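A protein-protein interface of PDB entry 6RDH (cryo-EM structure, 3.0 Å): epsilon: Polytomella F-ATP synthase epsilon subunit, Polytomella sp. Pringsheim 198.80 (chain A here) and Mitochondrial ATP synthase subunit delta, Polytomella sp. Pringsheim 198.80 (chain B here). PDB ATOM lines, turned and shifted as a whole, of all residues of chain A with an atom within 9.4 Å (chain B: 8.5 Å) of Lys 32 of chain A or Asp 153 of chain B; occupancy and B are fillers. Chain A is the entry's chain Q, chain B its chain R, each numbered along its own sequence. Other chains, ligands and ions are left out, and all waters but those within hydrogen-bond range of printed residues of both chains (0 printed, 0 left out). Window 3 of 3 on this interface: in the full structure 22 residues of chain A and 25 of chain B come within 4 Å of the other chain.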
ATOM      1  N   LEU A  26     -20.725   7.456  15.998  1.00  0.00           N
ATOM      2  CA  LEU A  26     -21.775   7.693  16.974  1.00  0.00           C
ATOM      3  C   LEU A  26     -23.132   7.868  16.316  1.00  0.00           C
ATOM      4  O   LEU A  26     -24.150   7.521  16.920  1.00  0.00           O
ATOM      5  CB  LEU A  26     -21.410   8.912  17.810  1.00  0.00           C
ATOM      6  CG  LEU A  26     -20.811   8.711  19.189  1.00  0.00           C
ATOM      7  CD1 LEU A  26     -19.768   7.641  19.178  1.00  0.00           C
ATOM      8  CD2 LEU A  26     -20.160   9.998  19.561  1.00  0.00           C
ATOM      9  N   LEU A  27     -23.174   8.403  15.097  1.00  0.00           N
ATOM     10  CA  LEU A  27     -24.412   8.354  14.331  1.00  0.00           C
ATOM     11  C   LEU A  27     -24.753   6.926  13.933  1.00  0.00           C
ATOM     12  O   LEU A  27     -25.931   6.563  13.885  1.00  0.00           O
ATOM     13  CB  LEU A  27     -24.310   9.234  13.089  1.00  0.00           C
ATOM     14  CG  LEU A  27     -25.564   9.341  12.222  1.00  0.00           C
ATOM     15  CD1 LEU A  27     -26.749   9.709  13.075  1.00  0.00           C
ATOM     16  CD2 LEU A  27     -25.398  10.341  11.113  1.00  0.00           C
ATOM     17  N   ARG A  28     -23.743   6.101  13.664  1.00  0.00           N
ATOM     18  CA  ARG A  28     -24.014   4.711  13.315  1.00  0.00           C
ATOM     19  C   ARG A  28     -24.466   3.884  14.515  1.00  0.00           C
ATOM     20  O   ARG A  28     -25.288   2.978  14.358  1.00  0.00           O
ATOM     21  CB  ARG A  28     -22.776   4.077  12.686  1.00  0.00           C
ATOM     22  CG  ARG A  28     -22.414   4.640  11.337  1.00  0.00           C
ATOM     23  CD  ARG A  28     -21.221   3.921  10.760  1.00  0.00           C
ATOM     24  NE  ARG A  28     -20.604   4.694   9.695  1.00  0.00           N
ATOM     25  CZ  ARG A  28     -19.405   5.251   9.790  1.00  0.00           C
ATOM     26  NH1 ARG A  28     -18.697   5.110  10.896  1.00  0.00           N
ATOM     27  NH2 ARG A  28     -18.916   5.945   8.776  1.00  0.00           N
ATOM     28  N   ASN A  29     -23.965   4.182  15.711  1.00  0.00           N
ATOM     29  CA  ASN A  29     -24.281   3.386  16.891  1.00  0.00           C
ATOM     30  C   ASN A  29     -25.687   3.613  17.432  1.00  0.00           C
ATOM     31  O   ASN A  29     -26.062   2.957  18.406  1.00  0.00           O
ATOM     32  CB  ASN A  29     -23.274   3.670  18.008  1.00  0.00           C
ATOM     33  CG  ASN A  29     -21.960   2.952  17.806  1.00  0.00           C
ATOM     34  OD1 ASN A  29     -20.890   3.524  18.013  1.00  0.00           O
ATOM     35  ND2 ASN A  29     -22.030   1.690  17.403  1.00  0.00           N
ATOM     36  N   VAL A  30     -26.458   4.541  16.865  1.00  0.00           N
ATOM     37  CA  VAL A  30     -27.853   4.739  17.244  1.00  0.00           C
ATOM     38  C   VAL A  30     -28.714   4.695  15.993  1.00  0.00           C
ATOM     39  O   VAL A  30     -29.827   5.231  15.961  1.00  0.00           O
ATOM     40  CB  VAL A  30     -28.063   6.054  18.018  1.00  0.00           C
ATOM     41  CG1 VAL A  30     -27.323   6.019  19.342  1.00  0.00           C
ATOM     42  CG2 VAL A  30     -27.585   7.237  17.195  1.00  0.00           C
ATOM     43  N   LEU A  31     -28.210   4.045  14.959  1.00  0.00           N
ATOM     44  CA  LEU A  31     -28.973   3.849  13.743  1.00  0.00           C
ATOM     45  C   LEU A  31     -29.917   2.662  13.932  1.00  0.00           C
ATOM     46  O   LEU A  31     -29.722   1.827  14.820  1.00  0.00           O
ATOM     47  CB  LEU A  31     -28.018   3.619  12.571  1.00  0.00           C
ATOM     48  CG  LEU A  31     -28.466   3.817  11.128  1.00  0.00           C
ATOM     49  CD1 LEU A  31     -28.710   5.265  10.890  1.00  0.00           C
ATOM     50  CD2 LEU A  31     -27.398   3.320  10.189  1.00  0.00           C
ATOM     51  N   LYS A  32     -30.957   2.607  13.099  1.00  0.00           N
ATOM     52  CA  LYS A  32     -31.913   1.504  13.146  1.00  0.00           C
ATOM     53  C   LYS A  32     -31.245   0.195  12.737  1.00  0.00           C
ATOM     54  O   LYS A  32     -30.502   0.147  11.753  1.00  0.00           O
ATOM     55  CB  LYS A  32     -33.098   1.787  12.228  1.00  0.00           C
ATOM     56  CG  LYS A  32     -34.290   0.882  12.436  1.00  0.00           C
ATOM     57  CD  LYS A  32     -34.971   1.154  13.759  1.00  0.00           C
ATOM     58  CE  LYS A  32     -35.698   2.485  13.733  1.00  0.00           C
ATOM     59  NZ  LYS A  32     -36.746   2.537  12.680  1.00  0.00           N
ATOM     60  N   GLU A  33     -31.539  -0.864  13.493  1.00  0.00           N
ATOM     61  CA  GLU A  33     -30.827  -2.135  13.359  1.00  0.00           C
ATOM     62  C   GLU A  33     -30.937  -2.827  11.991  1.00  0.00           C
ATOM     63  O   GLU A  33     -29.958  -3.495  11.610  1.00  0.00           O
ATOM     64  CB  GLU A  33     -31.274  -3.060  14.511  1.00  0.00           C
ATOM     65  CG  GLU A  33     -30.705  -4.473  14.516  1.00  0.00           C
ATOM     66  CD  GLU A  33     -29.226  -4.506  14.871  1.00  0.00           C
ATOM     67  OE1 GLU A  33     -28.840  -3.904  15.895  1.00  0.00           O
ATOM     68  OE2 GLU A  33     -28.448  -5.133  14.119  1.00  0.00           O
ATOM     69  N   PRO A  34     -32.027  -2.706  11.207  1.00  0.00           N
ATOM     70  CA  PRO A  34     -31.940  -3.128   9.795  1.00  0.00           C
ATOM     71  C   PRO A  34     -30.862  -2.432   8.974  1.00  0.00           C
ATOM     72  O   PRO A  34     -30.379  -3.020   8.000  1.00  0.00           O
ATOM     73  CB  PRO A  34     -33.336  -2.804   9.258  1.00  0.00           C
ATOM     74  CG  PRO A  34     -34.203  -3.068  10.405  1.00  0.00           C
ATOM     75  CD  PRO A  34     -33.444  -2.638  11.622  1.00  0.00           C
ATOM     76  N   PHE A  35     -30.466  -1.208   9.333  1.00  0.00           N
ATOM     77  CA  PHE A  35     -29.357  -0.528   8.682  1.00  0.00           C
ATOM     78  C   PHE A  35     -28.121  -0.383   9.556  1.00  0.00           C
ATOM     79  O   PHE A  35     -27.030  -0.175   9.015  1.00  0.00           O
ATOM     80  CB  PHE A  35     -29.787   0.867   8.217  1.00  0.00           C
ATOM     81  CG  PHE A  35     -30.904   0.856   7.224  1.00  0.00           C
ATOM     82  CD1 PHE A  35     -30.658   0.573   5.892  1.00  0.00           C
ATOM     83  CD2 PHE A  35     -32.198   1.143   7.617  1.00  0.00           C
ATOM     84  CE1 PHE A  35     -31.685   0.572   4.969  1.00  0.00           C
ATOM     85  CE2 PHE A  35     -33.229   1.149   6.702  1.00  0.00           C
ATOM     86  CZ  PHE A  35     -32.971   0.862   5.375  1.00  0.00           C
ATOM     87  N   LYS A  36     -28.271  -0.486  10.881  1.00  0.00           N
ATOM     88  CA  LYS A  36     -27.150  -0.288  11.796  1.00  0.00           C
ATOM     89  C   LYS A  36     -26.086  -1.358  11.619  1.00  0.00           C
ATOM     90  O   LYS A  36     -24.890  -1.059  11.670  1.00  0.00           O
ATOM     91  CB  LYS A  36     -27.650  -0.273  13.239  1.00  0.00           C
ATOM     92  CG  LYS A  36     -26.574  -0.187  14.306  1.00  0.00           C
ATOM     93  CD  LYS A  36     -27.189  -0.204  15.694  1.00  0.00           C
ATOM     94  CE  LYS A  36     -26.132  -0.117  16.772  1.00  0.00           C
ATOM     95  NZ  LYS A  36     -25.163  -1.233  16.669  1.00  0.00           N
ATOM     96  N   ALA A  37     -26.500  -2.602  11.372  1.00  0.00           N
ATOM     97  CA  ALA A  37     -25.539  -3.693  11.253  1.00  0.00           C
ATOM     98  C   ALA A  37     -24.731  -3.584   9.969  1.00  0.00           C
ATOM     99  O   ALA A  37     -23.513  -3.794   9.977  1.00  0.00           O
ATOM    100  CB  ALA A  37     -26.261  -5.037  11.313  1.00  0.00           C
ATOM    101  N   LYS A  38     -25.379  -3.247   8.859  1.00  0.00           N
ATOM    102  CA  LYS A  38     -24.645  -3.068   7.617  1.00  0.00           C
ATOM    103  C   LYS A  38     -23.893  -1.745   7.570  1.00  0.00           C
ATOM    104  O   LYS A  38     -23.029  -1.573   6.706  1.00  0.00           O
ATOM    105  CB  LYS A  38     -25.591  -3.184   6.425  1.00  0.00           C
ATOM    106  CG  LYS A  38     -26.780  -2.260   6.484  1.00  0.00           C
ATOM    107  CD  LYS A  38     -27.594  -2.346   5.211  1.00  0.00           C
ATOM    108  CE  LYS A  38     -26.744  -1.998   4.000  1.00  0.00           C
ATOM    109  NZ  LYS A  38     -26.044  -0.693   4.158  1.00  0.00           N
ATOM    110  N   ALA A  39     -24.196  -0.814   8.469  1.00  0.00           N
ATOM    111  CA  ALA A  39     -23.320   0.326   8.676  1.00  0.00           C
ATOM    112  C   ALA A  39     -22.115  -0.008   9.545  1.00  0.00           C
ATOM    113  O   ALA A  39     -21.173   0.782   9.594  1.00  0.00           O
ATOM    114  CB  ALA A  39     -24.096   1.484   9.301  1.00  0.00           C
ATOM    115  N   GLN A  40     -22.114  -1.157  10.227  1.00  0.00           N
ATOM    116  CA  GLN A  40     -20.899  -1.621  10.888  1.00  0.00           C
ATOM    117  C   GLN A  40     -19.928  -2.281   9.924  1.00  0.00           C
ATOM    118  O   GLN A  40     -18.843  -2.690  10.351  1.00  0.00           O
ATOM    119  CB  GLN A  40     -21.216  -2.600  12.018  1.00  0.00           C
ATOM    120  CG  GLN A  40     -22.194  -2.084  13.045  1.00  0.00           C
ATOM    121  CD  GLN A  40     -21.523  -1.529  14.276  1.00  0.00           C
ATOM    122  OE1 GLN A  40     -20.379  -1.083  14.226  1.00  0.00           O
ATOM    123  NE2 GLN A  40     -22.236  -1.545  15.393  1.00  0.00           N
ATOM    124  N   LYS B 126     -34.886  14.889   4.062  1.00  0.00           N
ATOM    125  CA  LYS B 126     -34.294  15.347   5.313  1.00  0.00           C
ATOM    126  C   LYS B 126     -33.116  14.438   5.629  1.00  0.00           C
ATOM    127  O   LYS B 126     -33.273  13.369   6.214  1.00  0.00           O
ATOM    128  CB  LYS B 126     -35.315  15.337   6.440  1.00  0.00           C
ATOM    129  CG  LYS B 126     -36.573  16.135   6.183  1.00  0.00           C
ATOM    130  CD  LYS B 126     -36.238  17.550   5.809  1.00  0.00           C
ATOM    131  CE  LYS B 126     -37.417  18.477   5.969  1.00  0.00           C
ATOM    132  NZ  LYS B 126     -37.884  18.500   7.381  1.00  0.00           N
ATOM    133  N   PHE B 127     -31.925  14.877   5.244  1.00  0.00           N
ATOM    134  CA  PHE B 127     -30.704  14.121   5.484  1.00  0.00           C
ATOM    135  C   PHE B 127     -30.028  14.641   6.741  1.00  0.00           C
ATOM    136  O   PHE B 127     -29.514  15.760   6.754  1.00  0.00           O
ATOM    137  CB  PHE B 127     -29.767  14.229   4.291  1.00  0.00           C
ATOM    138  CG  PHE B 127     -30.002  13.196   3.253  1.00  0.00           C
ATOM    139  CD1 PHE B 127     -29.882  11.857   3.566  1.00  0.00           C
ATOM    140  CD2 PHE B 127     -30.337  13.558   1.964  1.00  0.00           C
ATOM    141  CE1 PHE B 127     -30.094  10.900   2.617  1.00  0.00           C
ATOM    142  CE2 PHE B 127     -30.549  12.604   1.001  1.00  0.00           C
ATOM    143  CZ  PHE B 127     -30.428  11.271   1.328  1.00  0.00           C
ATOM    144  N   PHE B 128     -30.011  13.830   7.791  1.00  0.00           N
ATOM    145  CA  PHE B 128     -29.271  14.171   8.995  1.00  0.00           C
ATOM    146  C   PHE B 128     -27.811  13.790   8.800  1.00  0.00           C
ATOM    147  O   PHE B 128     -27.483  12.606   8.711  1.00  0.00           O
ATOM    148  CB  PHE B 128     -29.841  13.456  10.216  1.00  0.00           C
ATOM    149  CG  PHE B 128     -29.127  13.784  11.488  1.00  0.00           C
ATOM    150  CD1 PHE B 128     -29.391  14.963  12.153  1.00  0.00           C
ATOM    151  CD2 PHE B 128     -28.191  12.918  12.022  1.00  0.00           C
ATOM    152  CE1 PHE B 128     -28.734  15.275  13.319  1.00  0.00           C
ATOM    153  CE2 PHE B 128     -27.530  13.231  13.185  1.00  0.00           C
ATOM    154  CZ  PHE B 128     -27.805  14.406  13.835  1.00  0.00           C
ATOM    155  N   ALA B 150     -27.154   9.901   7.559  1.00  0.00           N
ATOM    156  CA  ALA B 150     -28.346   9.077   7.666  1.00  0.00           C
ATOM    157  C   ALA B 150     -29.597   9.909   7.431  1.00  0.00           C
ATOM    158  O   ALA B 150     -29.702  11.050   7.881  1.00  0.00           O
ATOM    159  CB  ALA B 150     -28.422   8.432   9.043  1.00  0.00           C
ATOM    160  N   THR B 151     -30.559   9.330   6.728  1.00  0.00           N
ATOM    161  CA  THR B 151     -31.853   9.986   6.687  1.00  0.00           C
ATOM    162  C   THR B 151     -32.599   9.702   7.986  1.00  0.00           C
ATOM    163  O   THR B 151     -32.246   8.806   8.754  1.00  0.00           O
ATOM    164  CB  THR B 151     -32.654   9.544   5.464  1.00  0.00           C
ATOM    165  OG1 THR B 151     -33.736  10.456   5.239  1.00  0.00           O
ATOM    166  CG2 THR B 151     -33.198   8.162   5.660  1.00  0.00           C
ATOM    167  N   LEU B 152     -33.634  10.494   8.245  1.00  0.00           N
ATOM    168  CA  LEU B 152     -34.222  10.525   9.578  1.00  0.00           C
ATOM    169  C   LEU B 152     -35.131   9.341   9.884  1.00  0.00           C
ATOM    170  O   LEU B 152     -35.397   9.087  11.063  1.00  0.00           O
ATOM    171  CB  LEU B 152     -34.987  11.831   9.768  1.00  0.00           C
ATOM    172  CG  LEU B 152     -34.059  12.978  10.144  1.00  0.00           C
ATOM    173  CD1 LEU B 152     -34.724  14.299   9.925  1.00  0.00           C
ATOM    174  CD2 LEU B 152     -33.644  12.838  11.593  1.00  0.00           C
ATOM    175  N   ASP B 153     -35.597   8.603   8.875  1.00  0.00           N
ATOM    176  CA  ASP B 153     -36.499   7.491   9.151  1.00  0.00           C
ATOM    177  C   ASP B 153     -35.757   6.278   9.696  1.00  0.00           C
ATOM    178  O   ASP B 153     -36.340   5.479  10.436  1.00  0.00           O
ATOM    179  CB  ASP B 153     -37.309   7.139   7.901  1.00  0.00           C
ATOM    180  CG  ASP B 153     -36.450   6.916   6.665  1.00  0.00           C
ATOM    181  OD1 ASP B 153     -36.802   7.485   5.610  1.00  0.00           O
ATOM    182  OD2 ASP B 153     -35.482   6.129   6.706  1.00  0.00           O
ATOM    183  N   GLN B 154     -34.482   6.115   9.338  1.00  0.00           N
ATOM    184  CA  GLN B 154     -33.698   4.966   9.773  1.00  0.00           C
ATOM    185  C   GLN B 154     -32.949   5.238  11.069  1.00  0.00           C
ATOM    186  O   GLN B 154     -31.887   4.657  11.308  1.00  0.00           O
ATOM    187  CB  GLN B 154     -32.729   4.520   8.678  1.00  0.00           C
ATOM    188  CG  GLN B 154     -31.752   5.563   8.174  1.00  0.00           C
ATOM    189  CD  GLN B 154     -31.314   5.304   6.746  1.00  0.00           C
ATOM    190  OE1 GLN B 154     -32.125   4.966   5.889  1.00  0.00           O
ATOM    191  NE2 GLN B 154     -30.021   5.434   6.490  1.00  0.00           N
ATOM    192  N   VAL B 155     -33.489   6.105  11.917  1.00  0.00           N
ATOM    193  CA  VAL B 155     -32.912   6.408  13.220  1.00  0.00           C
ATOM    194  C   VAL B 155     -33.831   5.838  14.286  1.00  0.00           C
ATOM    195  O   VAL B 155     -35.056   5.992  14.202  1.00  0.00           O
ATOM    196  CB  VAL B 155     -32.726   7.921  13.415  1.00  0.00           C
ATOM    197  CG1 VAL B 155     -31.772   8.186  14.561  1.00  0.00           C
ATOM    198  CG2 VAL B 155     -32.239   8.564  12.135  1.00  0.00           C
ATOM    199  N   ASP B 156     -33.247   5.168  15.278  1.00  0.00           N
ATOM    200  CA  ASP B 156     -34.187   4.805  16.323  1.00  0.00           C
ATOM    201  C   ASP B 156     -34.186   5.858  17.426  1.00  0.00           C
ATOM    202  O   ASP B 156     -33.134   6.400  17.778  1.00  0.00           O
ATOM    203  CB  ASP B 156     -33.847   3.434  16.908  1.00  0.00           C
ATOM    204  CG  ASP B 156     -32.481   3.388  17.552  1.00  0.00           C
ATOM    205  OD1 ASP B 156     -32.367   3.750  18.740  1.00  0.00           O
ATOM    206  OD2 ASP B 156     -31.519   2.974  16.877  1.00  0.00           O
ATOM    207  N   PRO B 157     -35.348   6.191  17.981  1.00  0.00           N
ATOM    208  CA  PRO B 157     -35.396   7.128  19.109  1.00  0.00           C
ATOM    209  C   PRO B 157     -35.157   6.495  20.472  1.00  0.00           C
ATOM    210  O   PRO B 157     -35.315   7.185  21.483  1.00  0.00           O
ATOM    211  CB  PRO B 157     -36.826   7.670  19.016  1.00  0.00           C
ATOM    212  CG  PRO B 157     -37.600   6.531  18.480  1.00  0.00           C
ATOM    213  CD  PRO B 157     -36.695   5.813  17.521  1.00  0.00           C
ATOM    214  N   ALA B 158     -34.769   5.224  20.531  1.00  0.00           N
ATOM    215  CA  ALA B 158     -34.617   4.534  21.804  1.00  0.00           C
ATOM    216  C   ALA B 158     -33.191   4.611  22.337  1.00  0.00           C
ATOM    217  O   ALA B 158     -32.985   4.831  23.535  1.00  0.00           O
ATOM    218  CB  ALA B 158     -35.048   3.073  21.663  1.00  0.00           C
ATOM    219  N   ALA B 159     -32.198   4.426  21.469  1.00  0.00           N
ATOM    220  CA  ALA B 159     -30.816   4.464  21.925  1.00  0.00           C
ATOM    221  C   ALA B 159     -30.301   5.882  22.110  1.00  0.00           C
ATOM    222  O   ALA B 159     -29.297   6.071  22.806  1.00  0.00           O
ATOM    223  CB  ALA B 159     -29.910   3.709  20.954  1.00  0.00           C
ATOM    224  N   LEU B 191     -29.754  15.229  17.377  1.00  0.00           N
ATOM    225  CA  LEU B 191     -30.541  14.156  16.789  1.00  0.00           C
ATOM    226  C   LEU B 191     -31.905  14.034  17.454  1.00  0.00           C
ATOM    227  O   LEU B 191     -32.911  13.821  16.773  1.00  0.00           O
ATOM    228  CB  LEU B 191     -29.763  12.849  16.885  1.00  0.00           C
ATOM    229  CG  LEU B 191     -30.246  11.672  16.056  1.00  0.00           C
ATOM    230  CD1 LEU B 191     -30.678  12.111  14.665  1.00  0.00           C
ATOM    231  CD2 LEU B 191     -29.114  10.685  15.979  1.00  0.00           C
ATOM    232  N   ALA B 194     -33.975  16.887  16.241  1.00  0.00           N
ATOM    233  CA  ALA B 194     -34.465  16.691  14.889  1.00  0.00           C
ATOM    234  C   ALA B 194     -35.227  15.392  14.697  1.00  0.00           C
ATOM    235  O   ALA B 194     -35.564  15.064  13.560  1.00  0.00           O
ATOM    236  CB  ALA B 194     -33.310  16.740  13.898  1.00  0.00           C
ATOM    237  N   VAL B 195     -35.458  14.616  15.751  1.00  0.00           N
ATOM    238  CA  VAL B 195     -36.339  13.462  15.643  1.00  0.00           C
ATOM    239  C   VAL B 195     -37.610  13.616  16.479  1.00  0.00           C
ATOM    240  O   VAL B 195     -38.621  12.972  16.158  1.00  0.00           O
ATOM    241  CB  VAL B 195     -35.602  12.147  15.993  1.00  0.00           C
ATOM    242  CG1 VAL B 195     -35.505  11.900  17.492  1.00  0.00           C
ATOM    243  CG2 VAL B 195     -36.204  10.964  15.254  1.00  0.00           C
ATOM    244  N   LYS B 198     -40.417  16.416  14.181  1.00  0.00           N
ATOM    245  CA  LYS B 198     -40.720  16.057  12.804  1.00  0.00           C
ATOM    246  C   LYS B 198     -42.221  15.977  12.567  1.00  0.00           C
ATOM    247  O   LYS B 198     -43.038  16.118  13.481  1.00  0.00           O
ATOM    248  CB  LYS B 198     -40.062  14.726  12.425  1.00  0.00           C
ATOM    249  CG  LYS B 198     -38.544  14.734  12.389  1.00  0.00           C
ATOM    250  CD  LYS B 198     -37.983  15.491  11.175  1.00  0.00           C
ATOM    251  CE  LYS B 198     -37.422  16.877  11.506  1.00  0.00           C
ATOM    252  NZ  LYS B 198     -36.840  17.544  10.307  1.00  0.00           N
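Among the printed residues, pairs that only touch across the chains: Leu 31 of chain A with Gln 154 of chain B, Phe 35 of chain A with Gln 154 of chain B, Lys 32 of chain A with Val 155 of chain B, Leu 27 of chain A with Phe 128 of chain B, Leu 31 of chain A with Ala 150 of chain B, Lys 32 of chain A with Asp 153 of chain B, Lys 32 of chain A with Asp 156 of chain B, Val 30 of chain A with Val 155 of chain B, Val 30 of chain A with Ala 159 of chain B, Leu 27 of chain A with Leu 191 of chain B, Val 30 of chain A with Leu 191 of chain B and Leu 27 of chain A with Ala 150 of chain B.
The side-chain carboxylate (OD2) of Asp 156 of chain B sits close to the backbone carbonyl oxygen (O) of Leu 31 of chain A (3.0 Å). The backbone NH of Asp 156 of chain B sits at hydrogen-bond distance from the backbone carbonyl oxygen of Val 30 of chain A (3.5 Å). The backbone carbonyl oxygen (O) of Gln 154 of chain B lies within hydrogen-bond range of the backbone NH (N) of Lys 32 of chain A (2.9 Å).
The side-chain carboxylate of Asp 156 of chain B lies within hydrogen-bond range of the backbone NH of Ala 159 of chain B (2.8 Å). OD1 of Asp 156 of chain B lies close to N of Ala 158 of chain B. The backbone NH (N) of Phe 128 of chain B sits at hydrogen-bond distance from the backbone carbonyl oxygen (O) of Ala 150 of chain B.
Of the 15 printed residues of chain A, 5 touch a printed residue of chain B. Printed residues of chain A that touch a printed residue of chain B: Leu 27, Val 30, Leu 31, Lys 32 and Phe 35. Hydrophobic or aromatic side chains of chain A that line the printed part of chain B: Leu 27, Val 30, Leu 31 and Phe 35. Along chain A the printed residues that touch a printed residue of chain B span positions 27 to 35. Of the 17 printed residues of chain B, 8 touch a printed residue of chain A. Printed residues of chain B that touch a printed residue of chain A: Phe 128, Ala 150, Asp 153, Gln 154, Val 155, Asp 156, Ala 159 and Leu 191. Hydrophobic or aromatic side chains of chain B within 4 Å of the printed part of chain A: Phe 128, Ala 150, Val 155, Ala 159 and Leu 191. Among the printed residues, no Asp or Glu carboxylate lies within 4 Å of a Lys or Arg side-chain nitrogen of the other chain.
Lys 32 of chain A touches just these residues of chain B: Asp 153 (3.7 Å), Gln 154 (2.9 Å), Val 155 (3.6 Å) and Asp 156 (3.8 Å). Asp 153 of chain B touches just one residue of chain A: Lys 32 (3.7 Å). Of the printed residues of chain B, Phe 35 of chain A touches Gln 154. Printed residues of chain A within 4 Å of Asp 156 of chain B: Val 30 (3.0 Å), Leu 31 (3.0 Å) and Lys 32 (3.8 Å). Printed residues of chain B within 4 Å of Val 30 of chain A: Val 155 (3.8 Å), Asp 156 (3.0 Å), Ala 159 (3.8 Å) and Leu 191 (3.96 Å). Glu 33 of chain A touches none of the printed residues of chain B. The nearest printed residue of chain B that does not touch Leu 27 of chain A is Val 155 of chain B (5.5 Å).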
